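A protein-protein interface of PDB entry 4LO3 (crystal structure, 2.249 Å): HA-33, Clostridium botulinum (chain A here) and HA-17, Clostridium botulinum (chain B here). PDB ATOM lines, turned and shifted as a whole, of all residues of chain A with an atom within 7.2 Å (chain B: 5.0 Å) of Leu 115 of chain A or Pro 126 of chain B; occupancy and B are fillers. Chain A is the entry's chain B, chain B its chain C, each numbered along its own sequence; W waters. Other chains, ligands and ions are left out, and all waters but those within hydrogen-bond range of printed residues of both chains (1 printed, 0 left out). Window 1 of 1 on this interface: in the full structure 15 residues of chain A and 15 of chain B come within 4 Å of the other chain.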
ATOM      1  N   TRP A  74      -4.657  12.086 -11.265  1.00  0.00           N
ATOM      2  CA  TRP A  74      -5.701  12.253 -10.251  1.00  0.00           C
ATOM      3  C   TRP A  74      -6.801  13.169 -10.787  1.00  0.00           C
ATOM      4  O   TRP A  74      -6.556  14.334 -11.132  1.00  0.00           O
ATOM      5  CB  TRP A  74      -5.122  12.845  -8.959  1.00  0.00           C
ATOM      6  CG  TRP A  74      -6.176  13.286  -7.969  1.00  0.00           C
ATOM      7  CD1 TRP A  74      -7.418  12.739  -7.791  1.00  0.00           C
ATOM      8  CD2 TRP A  74      -6.081  14.376  -7.030  1.00  0.00           C
ATOM      9  NE1 TRP A  74      -8.102  13.423  -6.811  1.00  0.00           N
ATOM     10  CE2 TRP A  74      -7.305  14.425  -6.324  1.00  0.00           C
ATOM     11  CE3 TRP A  74      -5.080  15.307  -6.722  1.00  0.00           C
ATOM     12  CZ2 TRP A  74      -7.559  15.376  -5.328  1.00  0.00           C
ATOM     13  CZ3 TRP A  74      -5.332  16.256  -5.728  1.00  0.00           C
ATOM     14  CH2 TRP A  74      -6.574  16.284  -5.047  1.00  0.00           C
ATOM     15  N   ALA A  76      -8.863  15.257  -9.738  1.00  0.00           N
ATOM     16  CA  ALA A  76      -9.237  16.228  -8.714  1.00  0.00           C
ATOM     17  C   ALA A  76     -10.504  16.980  -9.138  1.00  0.00           C
ATOM     18  O   ALA A  76     -10.604  17.419 -10.282  1.00  0.00           O
ATOM     19  CB  ALA A  76      -8.087  17.204  -8.496  1.00  0.00           C
ATOM     20  N   PRO A  77     -11.460  17.165  -8.209  1.00  0.00           N
ATOM     21  CA  PRO A  77     -11.334  16.855  -6.781  1.00  0.00           C
ATOM     22  C   PRO A  77     -11.852  15.479  -6.383  1.00  0.00           C
ATOM     23  O   PRO A  77     -11.926  15.217  -5.179  1.00  0.00           O
ATOM     24  CB  PRO A  77     -12.243  17.899  -6.136  1.00  0.00           C
ATOM     25  CG  PRO A  77     -13.396  18.015  -7.156  1.00  0.00           C
ATOM     26  CD  PRO A  77     -12.744  17.838  -8.516  1.00  0.00           C
ATOM     27  N   THR A  78     -12.215  14.631  -7.343  1.00  0.00           N
ATOM     28  CA  THR A  78     -12.816  13.333  -7.019  1.00  0.00           C
ATOM     29  C   THR A  78     -11.819  12.338  -6.399  1.00  0.00           C
ATOM     30  O   THR A  78     -10.622  12.597  -6.355  1.00  0.00           O
ATOM     31  CB  THR A  78     -13.419  12.667  -8.274  1.00  0.00           C
ATOM     32  OG1 THR A  78     -12.371  12.053  -9.036  1.00  0.00           O
ATOM     33  CG2 THR A  78     -14.164  13.693  -9.136  1.00  0.00           C
ATOM     34  N   HIS A  79     -12.318  11.192  -5.937  1.00  0.00           N
ATOM     35  CA  HIS A  79     -11.456  10.133  -5.415  1.00  0.00           C
ATOM     36  C   HIS A  79     -10.866   9.253  -6.531  1.00  0.00           C
ATOM     37  O   HIS A  79     -10.210   8.252  -6.245  1.00  0.00           O
ATOM     38  CB  HIS A  79     -12.230   9.222  -4.455  1.00  0.00           C
ATOM     39  CG  HIS A  79     -12.840   9.933  -3.282  1.00  0.00           C
ATOM     40  ND1 HIS A  79     -13.907  10.800  -3.414  1.00  0.00           N
ATOM     41  CD2 HIS A  79     -12.548   9.887  -1.967  1.00  0.00           C
ATOM     42  CE1 HIS A  79     -14.232  11.263  -2.222  1.00  0.00           C
ATOM     43  NE2 HIS A  79     -13.430  10.731  -1.324  1.00  0.00           N
ATOM     44  N   TRP A  94       3.692  13.156  -9.119  1.00  0.00           N
ATOM     45  CA  TRP A  94       3.629  12.315  -7.927  1.00  0.00           C
ATOM     46  C   TRP A  94       4.956  12.348  -7.187  1.00  0.00           C
ATOM     47  O   TRP A  94       6.031  12.313  -7.805  1.00  0.00           O
ATOM     48  CB  TRP A  94       3.299  10.869  -8.337  1.00  0.00           C
ATOM     49  CG  TRP A  94       2.008  10.787  -9.092  1.00  0.00           C
ATOM     50  CD1 TRP A  94       1.844  10.823 -10.460  1.00  0.00           C
ATOM     51  CD2 TRP A  94       0.687  10.690  -8.532  1.00  0.00           C
ATOM     52  NE1 TRP A  94       0.505  10.752 -10.771  1.00  0.00           N
ATOM     53  CE2 TRP A  94      -0.224  10.667  -9.612  1.00  0.00           C
ATOM     54  CE3 TRP A  94       0.190  10.625  -7.221  1.00  0.00           C
ATOM     55  CZ2 TRP A  94      -1.612  10.578  -9.423  1.00  0.00           C
ATOM     56  CZ3 TRP A  94      -1.199  10.538  -7.033  1.00  0.00           C
ATOM     57  CH2 TRP A  94      -2.078  10.518  -8.127  1.00  0.00           C
ATOM     58  N   ILE A 106       5.451   5.212  -0.717  1.00  0.00           N
ATOM     59  CA  ILE A 106       4.210   5.956  -0.672  1.00  0.00           C
ATOM     60  C   ILE A 106       4.184   6.879  -1.889  1.00  0.00           C
ATOM     61  O   ILE A 106       5.196   7.522  -2.237  1.00  0.00           O
ATOM     62  CB  ILE A 106       4.129   6.763   0.649  1.00  0.00           C
ATOM     63  CG1 ILE A 106       3.905   5.775   1.803  1.00  0.00           C
ATOM     64  CG2 ILE A 106       3.039   7.812   0.582  1.00  0.00           C
ATOM     65  CD1 ILE A 106       4.090   6.377   3.161  1.00  0.00           C
ATOM     66  N   ILE A 107       3.046   6.935  -2.565  1.00  0.00           N
ATOM     67  CA  ILE A 107       2.942   7.740  -3.781  1.00  0.00           C
ATOM     68  C   ILE A 107       1.964   8.911  -3.574  1.00  0.00           C
ATOM     69  O   ILE A 107       0.744   8.735  -3.627  1.00  0.00           O
ATOM     70  CB  ILE A 107       2.526   6.860  -4.964  1.00  0.00           C
ATOM     71  CG1 ILE A 107       3.542   5.714  -5.125  1.00  0.00           C
ATOM     72  CG2 ILE A 107       2.428   7.675  -6.251  1.00  0.00           C
ATOM     73  CD1 ILE A 107       3.136   4.673  -6.165  1.00  0.00           C
ATOM     74  N   ALA A 108       2.521  10.099  -3.329  1.00  0.00           N
ATOM     75  CA  ALA A 108       1.751  11.276  -2.929  1.00  0.00           C
ATOM     76  C   ALA A 108       1.485  12.178  -4.123  1.00  0.00           C
ATOM     77  O   ALA A 108       2.355  12.339  -4.994  1.00  0.00           O
ATOM     78  CB  ALA A 108       2.517  12.063  -1.846  1.00  0.00           C
ATOM     79  N   SER A 109       0.300  12.783  -4.174  1.00  0.00           N
ATOM     80  CA  SER A 109      -0.014  13.696  -5.278  1.00  0.00           C
ATOM     81  C   SER A 109       0.784  14.989  -5.175  1.00  0.00           C
ATOM     82  O   SER A 109       0.837  15.618  -4.118  1.00  0.00           O
ATOM     83  CB  SER A 109      -1.500  14.061  -5.278  1.00  0.00           C
ATOM     84  OG  SER A 109      -1.761  15.010  -6.310  1.00  0.00           O
ATOM     85  N   TYR A 110       1.380  15.406  -6.280  1.00  0.00           N
ATOM     86  CA  TYR A 110       2.057  16.690  -6.302  1.00  0.00           C
ATOM     87  C   TYR A 110       1.052  17.823  -6.142  1.00  0.00           C
ATOM     88  O   TYR A 110       1.373  18.862  -5.547  1.00  0.00           O
ATOM     89  CB  TYR A 110       2.853  16.867  -7.601  1.00  0.00           C
ATOM     90  CG  TYR A 110       3.531  18.213  -7.720  1.00  0.00           C
ATOM     91  CD1 TYR A 110       4.656  18.518  -6.951  1.00  0.00           C
ATOM     92  CD2 TYR A 110       3.056  19.180  -8.598  1.00  0.00           C
ATOM     93  CE1 TYR A 110       5.284  19.751  -7.052  1.00  0.00           C
ATOM     94  CE2 TYR A 110       3.684  20.424  -8.712  1.00  0.00           C
ATOM     95  CZ  TYR A 110       4.793  20.703  -7.929  1.00  0.00           C
ATOM     96  OH  TYR A 110       5.415  21.932  -8.035  1.00  0.00           O
ATOM     97  N   LYS A 111      -0.166  17.638  -6.655  1.00  0.00           N
ATOM     98  CA  LYS A 111      -1.159  18.715  -6.572  1.00  0.00           C
ATOM     99  C   LYS A 111      -1.658  18.929  -5.140  1.00  0.00           C
ATOM    100  O   LYS A 111      -2.016  20.050  -4.755  1.00  0.00           O
ATOM    101  CB  LYS A 111      -2.349  18.465  -7.506  1.00  0.00           C
ATOM    102  CG  LYS A 111      -3.296  19.659  -7.595  1.00  0.00           C
ATOM    103  CD  LYS A 111      -4.520  19.361  -8.430  1.00  0.00           C
ATOM    104  CE  LYS A 111      -5.332  20.638  -8.659  1.00  0.00           C
ATOM    105  NZ  LYS A 111      -4.614  21.577  -9.567  1.00  0.00           N
ATOM    106  N   ASN A 112      -1.684  17.852  -4.358  1.00  0.00           N
ATOM    107  CA  ASN A 112      -2.045  17.917  -2.936  1.00  0.00           C
ATOM    108  C   ASN A 112      -1.331  16.798  -2.196  1.00  0.00           C
ATOM    109  O   ASN A 112      -1.835  15.676  -2.111  1.00  0.00           O
ATOM    110  CB  ASN A 112      -3.559  17.778  -2.745  1.00  0.00           C
ATOM    111  CG  ASN A 112      -4.000  18.060  -1.313  1.00  0.00           C
ATOM    112  OD1 ASN A 112      -3.258  17.806  -0.341  1.00  0.00           O
ATOM    113  ND2 ASN A 112      -5.214  18.599  -1.170  1.00  0.00           N
ATOM    114  N   PRO A 113      -0.151  17.108  -1.651  1.00  0.00           N
ATOM    115  CA  PRO A 113       0.746  16.115  -1.047  1.00  0.00           C
ATOM    116  C   PRO A 113       0.180  15.491   0.229  1.00  0.00           C
ATOM    117  O   PRO A 113       0.752  14.519   0.721  1.00  0.00           O
ATOM    118  CB  PRO A 113       2.029  16.909  -0.748  1.00  0.00           C
ATOM    119  CG  PRO A 113       1.876  18.214  -1.432  1.00  0.00           C
ATOM    120  CD  PRO A 113       0.415  18.463  -1.635  1.00  0.00           C
ATOM    121  N   ASN A 114      -0.914  16.033   0.761  1.00  0.00           N
ATOM    122  CA  ASN A 114      -1.617  15.359   1.851  1.00  0.00           C
ATOM    123  C   ASN A 114      -2.332  14.098   1.378  1.00  0.00           C
ATOM    124  O   ASN A 114      -2.787  13.290   2.196  1.00  0.00           O
ATOM    125  CB  ASN A 114      -2.650  16.290   2.491  1.00  0.00           C
ATOM    126  CG  ASN A 114      -2.011  17.462   3.191  1.00  0.00           C
ATOM    127  OD1 ASN A 114      -1.467  17.316   4.291  1.00  0.00           O
ATOM    128  ND2 ASN A 114      -2.071  18.636   2.565  1.00  0.00           N
ATOM    129  N   LEU A 115      -2.447  13.931   0.063  1.00  0.00           N
ATOM    130  CA  LEU A 115      -3.188  12.798  -0.478  1.00  0.00           C
ATOM    131  C   LEU A 115      -2.259  11.840  -1.172  1.00  0.00           C
ATOM    132  O   LEU A 115      -1.393  12.257  -1.959  1.00  0.00           O
ATOM    133  CB  LEU A 115      -4.249  13.285  -1.486  1.00  0.00           C
ATOM    134  CG  LEU A 115      -5.321  14.110  -0.777  1.00  0.00           C
ATOM    135  CD1 LEU A 115      -6.334  14.636  -1.793  1.00  0.00           C
ATOM    136  CD2 LEU A 115      -6.006  13.233   0.281  1.00  0.00           C
ATOM    137  N   VAL A 116      -2.442  10.552  -0.894  1.00  0.00           N
ATOM    138  CA  VAL A 116      -1.561   9.530  -1.458  1.00  0.00           C
ATOM    139  C   VAL A 116      -2.398   8.409  -2.066  1.00  0.00           C
ATOM    140  O   VAL A 116      -3.583   8.246  -1.740  1.00  0.00           O
ATOM    141  CB  VAL A 116      -0.587   8.966  -0.382  1.00  0.00           C
ATOM    142  CG1 VAL A 116       0.085  10.113   0.379  1.00  0.00           C
ATOM    143  CG2 VAL A 116      -1.347   8.077   0.611  1.00  0.00           C
ATOM    144  N   LEU A 117      -1.787   7.650  -2.965  1.00  0.00           N
ATOM    145  CA  LEU A 117      -2.470   6.531  -3.585  1.00  0.00           C
ATOM    146  C   LEU A 117      -2.832   5.478  -2.545  1.00  0.00           C
ATOM    147  O   LEU A 117      -2.047   5.173  -1.620  1.00  0.00           O
ATOM    148  CB  LEU A 117      -1.606   5.903  -4.691  1.00  0.00           C
ATOM    149  CG  LEU A 117      -1.416   6.698  -5.981  1.00  0.00           C
ATOM    150  CD1 LEU A 117      -0.657   5.862  -7.046  1.00  0.00           C
ATOM    151  CD2 LEU A 117      -2.765   7.177  -6.550  1.00  0.00           C
ATOM    152  N   LYS A 127      -7.605   4.693  -5.299  1.00  0.00           N
ATOM    153  CA  LYS A 127      -8.240   5.915  -4.840  1.00  0.00           C
ATOM    154  C   LYS A 127      -7.219   6.701  -4.019  1.00  0.00           C
ATOM    155  O   LYS A 127      -6.014   6.519  -4.195  1.00  0.00           O
ATOM    156  CB  LYS A 127      -9.552   5.631  -4.089  1.00  0.00           C
ATOM    157  CG  LYS A 127      -9.468   4.569  -2.999  1.00  0.00           C
ATOM    158  CD  LYS A 127     -10.873   4.152  -2.516  1.00  0.00           C
ATOM    159  CE  LYS A 127     -10.804   3.240  -1.279  1.00  0.00           C
ATOM    160  NZ  LYS A 127     -12.142   2.856  -0.718  1.00  0.00           N
ATOM    161  N   LEU A 128      -7.675   7.579  -3.141  1.00  0.00           N
ATOM    162  CA  LEU A 128      -6.736   8.431  -2.424  1.00  0.00           C
ATOM    163  C   LEU A 128      -7.022   8.417  -0.943  1.00  0.00           C
ATOM    164  O   LEU A 128      -8.129   8.124  -0.513  1.00  0.00           O
ATOM    165  CB  LEU A 128      -6.809   9.873  -2.929  1.00  0.00           C
ATOM    166  CG  LEU A 128      -6.241  10.186  -4.306  1.00  0.00           C
ATOM    167  CD1 LEU A 128      -6.474  11.649  -4.581  1.00  0.00           C
ATOM    168  CD2 LEU A 128      -4.737   9.871  -4.412  1.00  0.00           C
ATOM    169  N   SER A 129      -6.006   8.735  -0.157  1.00  0.00           N
ATOM    170  CA  SER A 129      -6.162   8.805   1.280  1.00  0.00           C
ATOM    171  C   SER A 129      -5.134   9.784   1.823  1.00  0.00           C
ATOM    172  O   SER A 129      -4.090  10.033   1.194  1.00  0.00           O
ATOM    173  CB  SER A 129      -5.958   7.410   1.895  1.00  0.00           C
ATOM    174  OG  SER A 129      -5.944   7.446   3.313  1.00  0.00           O
ATOM    175  N   THR A 130      -5.445  10.358   2.980  1.00  0.00           N
ATOM    176  CA  THR A 130      -4.433  11.054   3.744  1.00  0.00           C
ATOM    177  C   THR A 130      -3.502   9.988   4.323  1.00  0.00           C
ATOM    178  O   THR A 130      -3.842   8.797   4.340  1.00  0.00           O
ATOM    179  CB  THR A 130      -5.068  11.915   4.847  1.00  0.00           C
ATOM    180  OG1 THR A 130      -5.923  11.093   5.652  1.00  0.00           O
ATOM    181  CG2 THR A 130      -5.891  13.022   4.208  1.00  0.00           C
ATOM    182  N   LEU A 131      -2.321  10.402   4.771  1.00  0.00           N
ATOM    183  CA  LEU A 131      -1.308   9.458   5.241  1.00  0.00           C
ATOM    184  C   LEU A 131      -1.726   8.701   6.497  1.00  0.00           C
ATOM    185  O   LEU A 131      -2.292   9.279   7.413  1.00  0.00           O
ATOM    186  CB  LEU A 131      -0.007  10.197   5.539  1.00  0.00           C
ATOM    187  CG  LEU A 131       0.981  10.366   4.406  1.00  0.00           C
ATOM    188  CD1 LEU A 131       2.076  11.325   4.859  1.00  0.00           C
ATOM    189  CD2 LEU A 131       1.565   9.006   4.065  1.00  0.00           C
ATOM    190  N   SER B  32     -16.889  14.123  -3.708  1.00  0.00           N
ATOM    191  CA  SER B  32     -16.084  15.120  -3.005  1.00  0.00           C
ATOM    192  C   SER B  32     -16.801  16.442  -2.857  1.00  0.00           C
ATOM    193  O   SER B  32     -17.819  16.693  -3.503  1.00  0.00           O
ATOM    194  CB  SER B  32     -14.761  15.375  -3.737  1.00  0.00           C
ATOM    195  OG  SER B  32     -14.018  14.192  -3.848  1.00  0.00           O
ATOM    196  N   LEU B  33     -16.236  17.290  -2.003  1.00  0.00           N
ATOM    197  CA  LEU B  33     -16.703  18.651  -1.818  1.00  0.00           C
ATOM    198  C   LEU B  33     -15.602  19.532  -2.380  1.00  0.00           C
ATOM    199  O   LEU B  33     -14.413  19.277  -2.137  1.00  0.00           O
ATOM    200  CB  LEU B  33     -16.896  18.969  -0.320  1.00  0.00           C
ATOM    201  CG  LEU B  33     -18.222  18.496   0.295  1.00  0.00           C
ATOM    202  CD1 LEU B  33     -19.425  19.069  -0.505  1.00  0.00           C
ATOM    203  CD2 LEU B  33     -18.297  16.952   0.368  1.00  0.00           C
ATOM    204  N   THR B  34     -15.979  20.565  -3.123  1.00  0.00           N
ATOM    205  CA  THR B  34     -14.989  21.464  -3.695  1.00  0.00           C
ATOM    206  C   THR B  34     -15.571  22.857  -3.833  1.00  0.00           C
ATOM    207  O   THR B  34     -16.789  23.043  -3.698  1.00  0.00           O
ATOM    208  CB  THR B  34     -14.499  20.962  -5.076  1.00  0.00           C
ATOM    209  OG1 THR B  34     -13.230  21.554  -5.384  1.00  0.00           O
ATOM    210  CG2 THR B  34     -15.522  21.305  -6.193  1.00  0.00           C
ATOM    211  N   PHE B  74     -10.954   8.262   4.767  1.00  0.00           N
ATOM    212  CA  PHE B  74      -9.816   8.536   3.885  1.00  0.00           C
ATOM    213  C   PHE B  74      -9.342   9.991   3.986  1.00  0.00           C
ATOM    214  O   PHE B  74      -8.474  10.425   3.223  1.00  0.00           O
ATOM    215  CB  PHE B  74     -10.163   8.153   2.441  1.00  0.00           C
ATOM    216  CG  PHE B  74     -10.653   6.740   2.310  1.00  0.00           C
ATOM    217  CD1 PHE B  74      -9.747   5.690   2.194  1.00  0.00           C
ATOM    218  CD2 PHE B  74     -12.020   6.453   2.349  1.00  0.00           C
ATOM    219  CE1 PHE B  74     -10.193   4.372   2.101  1.00  0.00           C
ATOM    220  CE2 PHE B  74     -12.478   5.140   2.263  1.00  0.00           C
ATOM    221  CZ  PHE B  74     -11.566   4.095   2.141  1.00  0.00           C
ATOM    222  N   PHE B  76     -11.294  12.691   3.674  1.00  0.00           N
ATOM    223  CA  PHE B  76     -12.119  13.586   2.864  1.00  0.00           C
ATOM    224  C   PHE B  76     -13.382  14.009   3.590  1.00  0.00           C
ATOM    225  O   PHE B  76     -14.046  13.168   4.210  1.00  0.00           O
ATOM    226  CB  PHE B  76     -12.605  12.854   1.615  1.00  0.00           C
ATOM    227  CG  PHE B  76     -11.584  12.724   0.533  1.00  0.00           C
ATOM    228  CD1 PHE B  76     -10.566  11.796   0.633  1.00  0.00           C
ATOM    229  CD2 PHE B  76     -11.683  13.492  -0.618  1.00  0.00           C
ATOM    230  CE1 PHE B  76      -9.628  11.665  -0.394  1.00  0.00           C
ATOM    231  CE2 PHE B  76     -10.755  13.364  -1.640  1.00  0.00           C
ATOM    232  CZ  PHE B  76      -9.726  12.452  -1.528  1.00  0.00           C
ATOM    233  N   ASP B 114     -10.212  21.573   5.904  1.00  0.00           N
ATOM    234  CA  ASP B 114      -8.935  22.088   5.474  1.00  0.00           C
ATOM    235  C   ASP B 114      -8.908  22.059   3.964  1.00  0.00           C
ATOM    236  O   ASP B 114      -9.179  21.025   3.347  1.00  0.00           O
ATOM    237  CB  ASP B 114      -7.819  21.225   6.074  1.00  0.00           C
ATOM    238  CG  ASP B 114      -6.423  21.804   5.836  1.00  0.00           C
ATOM    239  OD1 ASP B 114      -6.071  22.096   4.662  1.00  0.00           O
ATOM    240  OD2 ASP B 114      -5.670  21.961   6.830  1.00  0.00           O
ATOM    241  N   ILE B 115      -8.609  23.200   3.361  1.00  0.00           N
ATOM    242  CA  ILE B 115      -8.499  23.248   1.910  1.00  0.00           C
ATOM    243  C   ILE B 115      -7.074  23.626   1.516  1.00  0.00           C
ATOM    244  O   ILE B 115      -6.533  24.633   2.001  1.00  0.00           O
ATOM    245  CB  ILE B 115      -9.545  24.206   1.262  1.00  0.00           C
ATOM    246  CG1 ILE B 115      -9.585  24.028  -0.265  1.00  0.00           C
ATOM    247  CG2 ILE B 115      -9.322  25.670   1.683  1.00  0.00           C
ATOM    248  CD1 ILE B 115     -10.363  22.774  -0.714  1.00  0.00           C
ATOM    249  N   SER B 124     -10.182  22.991  -7.892  1.00  0.00           N
ATOM    250  CA  SER B 124     -10.148  21.530  -8.042  1.00  0.00           C
ATOM    251  C   SER B 124      -9.652  20.780  -6.808  1.00  0.00           C
ATOM    252  O   SER B 124      -9.549  19.545  -6.846  1.00  0.00           O
ATOM    253  CB  SER B 124      -9.335  21.097  -9.277  1.00  0.00           C
ATOM    254  OG  SER B 124      -9.816  21.724 -10.460  1.00  0.00           O
ATOM    255  N   GLN B 125      -9.347  21.497  -5.725  1.00  0.00           N
ATOM    256  CA  GLN B 125      -8.975  20.833  -4.471  1.00  0.00           C
ATOM    257  C   GLN B 125     -10.211  20.275  -3.748  1.00  0.00           C
ATOM    258  O   GLN B 125     -11.243  20.951  -3.645  1.00  0.00           O
ATOM    259  CB  GLN B 125      -8.232  21.809  -3.537  1.00  0.00           C
ATOM    260  CG  GLN B 125      -6.839  22.234  -4.013  1.00  0.00           C
ATOM    261  CD  GLN B 125      -5.831  21.080  -4.063  1.00  0.00           C
ATOM    262  OE1 GLN B 125      -6.046  20.019  -3.482  1.00  0.00           O
ATOM    263  NE2 GLN B 125      -4.718  21.296  -4.759  1.00  0.00           N
ATOM    264  N   PRO B 126     -10.111  19.042  -3.228  1.00  0.00           N
ATOM    265  CA  PRO B 126     -11.208  18.534  -2.401  1.00  0.00           C
ATOM    266  C   PRO B 126     -11.048  19.054  -0.968  1.00  0.00           C
ATOM    267  O   PRO B 126      -9.915  19.254  -0.496  1.00  0.00           O
ATOM    268  CB  PRO B 126     -10.977  17.021  -2.410  1.00  0.00           C
ATOM    269  CG  PRO B 126      -9.431  16.895  -2.504  1.00  0.00           C
ATOM    270  CD  PRO B 126      -8.963  18.112  -3.289  1.00  0.00           C
ATOM    271  N   LEU B 127     -12.164  19.279  -0.283  1.00  0.00           N
ATOM    272  CA  LEU B 127     -12.121  19.669   1.115  1.00  0.00           C
ATOM    273  C   LEU B 127     -11.759  18.448   1.970  1.00  0.00           C
ATOM    274  O   LEU B 127     -12.404  17.380   1.881  1.00  0.00           O
ATOM    275  CB  LEU B 127     -13.471  20.259   1.527  1.00  0.00           C
ATOM    276  CG  LEU B 127     -13.609  20.898   2.908  1.00  0.00           C
ATOM    277  CD1 LEU B 127     -12.669  22.104   3.044  1.00  0.00           C
ATOM    278  CD2 LEU B 127     -15.091  21.290   3.138  1.00  0.00           C
ATOM    279  N   LEU B 128     -10.708  18.590   2.781  1.00  0.00           N
ATOM    280  CA  LEU B 128     -10.252  17.491   3.634  1.00  0.00           C
ATOM    281  C   LEU B 128     -10.540  17.748   5.120  1.00  0.00           C
ATOM    282  O   LEU B 128     -10.990  18.834   5.508  1.00  0.00           O
ATOM    283  CB  LEU B 128      -8.753  17.244   3.427  1.00  0.00           C
ATOM    284  CG  LEU B 128      -8.307  17.024   1.970  1.00  0.00           C
ATOM    285  CD1 LEU B 128      -6.793  16.739   1.895  1.00  0.00           C
ATOM    286  CD2 LEU B 128      -9.119  15.891   1.318  1.00  0.00           C
HETATM  287  O   HOH W   1      -7.424  20.213   0.210  1.00  0.00           O
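O of Leu 128 of chain B is in hydrogen-bond range of N of Asp 114 of chain B, 2.9 Å away. NE1 of Trp 74 of chain A lies within hydrogen-bond range of O of Thr 78 of chain A, at 2.7 Å. The side-chain hydroxyl of Thr 34 of chain B sits at hydrogen-bond distance from the backbone carbonyl oxygen of Gln 125 of chain B (2.7 Å). The backbone NH (N) of Asn 114 of chain A lies close to the side-chain amide oxygen (OD1) of Asn 112 of chain A, 3.1 Å away. The backbone carbonyl oxygen of Ser 129 of chain A is in hydrogen-bond range of the backbone NH of Val 116 of chain A (2.7 Å). The backbone NH (N) of Ser 109 of chain A is in hydrogen-bond range of the backbone carbonyl oxygen (O) of Leu 115 of chain A (2.8 Å).
Of the printed residues of chain B, Leu 115 of chain A touches Pro 126 (3.9 Å) and Leu 128 (3.9 Å). Pro 126 of chain B touches just these residues of chain A: Trp 74, Pro 77 and Leu 115. Of the printed residues of chain B, Leu 128 of chain A touches Phe 74 (3.6 Å) and Phe 76 (3.8 Å). Of the printed residues of chain B, Trp 74 of chain A touches Pro 126. Printed residues of chain A within 4 Å of Phe 74 of chain B: Lys 127 (3.2 Å), Leu 128 (3.6 Å), Ser 129 (3.4 Å) and Thr 130 (3.0 Å). Of the printed residues of chain A, Ser 32 of chain B touches Pro 77, Thr 78 and His 79. Asp 114 of chain B touches none of the printed residues of chain A. The nearest residue of chain A that does not touch Pro 126 of chain B is Asn 112 of chain A (4.3 Å).
Of the 12 printed residues of chain B, 8 touch a printed residue of chain A. Printed residues of chain B that touch a printed residue of chain A: Ser 32, Thr 34, Phe 74, Phe 76, Ser 124, Gln 125, Pro 126 and Leu 128. Hydrophobic or aromatic side chains of chain B within 4 Å of the printed part of chain A: Phe 74, Phe 76, Pro 126 and Leu 128. Hydrophobic or aromatic side chains of chain A within 4 Å of the printed part of chain B: Trp 74, Ala 76, Pro 77, His 79 and Leu 115. Among the printed residues, 20 pairs touch across the chains. Among the printed residues, no Asp or Glu carboxylate lies within 4 Å of a Lys or Arg side-chain nitrogen of the other chain.
Water W1 lies within hydrogen-bond range of the backbone carbonyl oxygen (O) of Pro 126 of chain B (2.8 Å) and the side-chain amide nitrogen (ND2) of Asn 112 of chain A (3.1 Å).
Ala 76 of chain A touches Ser 124 of chain B (CB to O, 3.2 Å). Pro 126 of chain B touches Pro 77 of chain A. Thr 78 of chain A touches Ser 32 of chain B. His 79 of chain A touches Phe 76 of chain B (NE2 to CG, 3.3 Å). Asn 112 of chain A touches Leu 128 of chain B. CD1 of Leu 115 of chain A touches CG of Pro 126 of chain B, at 3.9 Å. CD2 of Leu 115 of chain A touches CD1 of Leu 128 of chain B (3.9 Å). NZ of Lys 127 of chain A touches CZ of Phe 74 of chain B (3.2 Å). Leu 128 of chain A touches Phe 76 of chain B (O to CE1, 3.8 Å). CA of Ser 129 of chain A touches O of Phe 74 of chain B (3.4 Å).
The backbone nitrogen (N) of Pro 77 of chain A lies close to the backbone carbonyl oxygen (O) of Ser 124 of chain B (3.3 Å). The backbone NH of Thr 130 of chain A sits at hydrogen-bond distance from the backbone carbonyl oxygen of Phe 74 of chain B (3.0 Å). OE1 of Gln 125 of chain B is in hydrogen-bond range of ND2 of Asn 112 of chain A, at 2.8 Å. O of Lys 111 of chain A is in hydrogen-bond range of NE2 of Gln 125 of chain B (3.0 Å). The backbone carbonyl oxygen (O) of Pro 77 of chain A sits at hydrogen-bond distance from the side-chain hydroxyl (OG) of Ser 32 of chain B. OG of Ser 32 of chain B lies close to ND1 of His 79 of chain A, 3.4 Å away.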
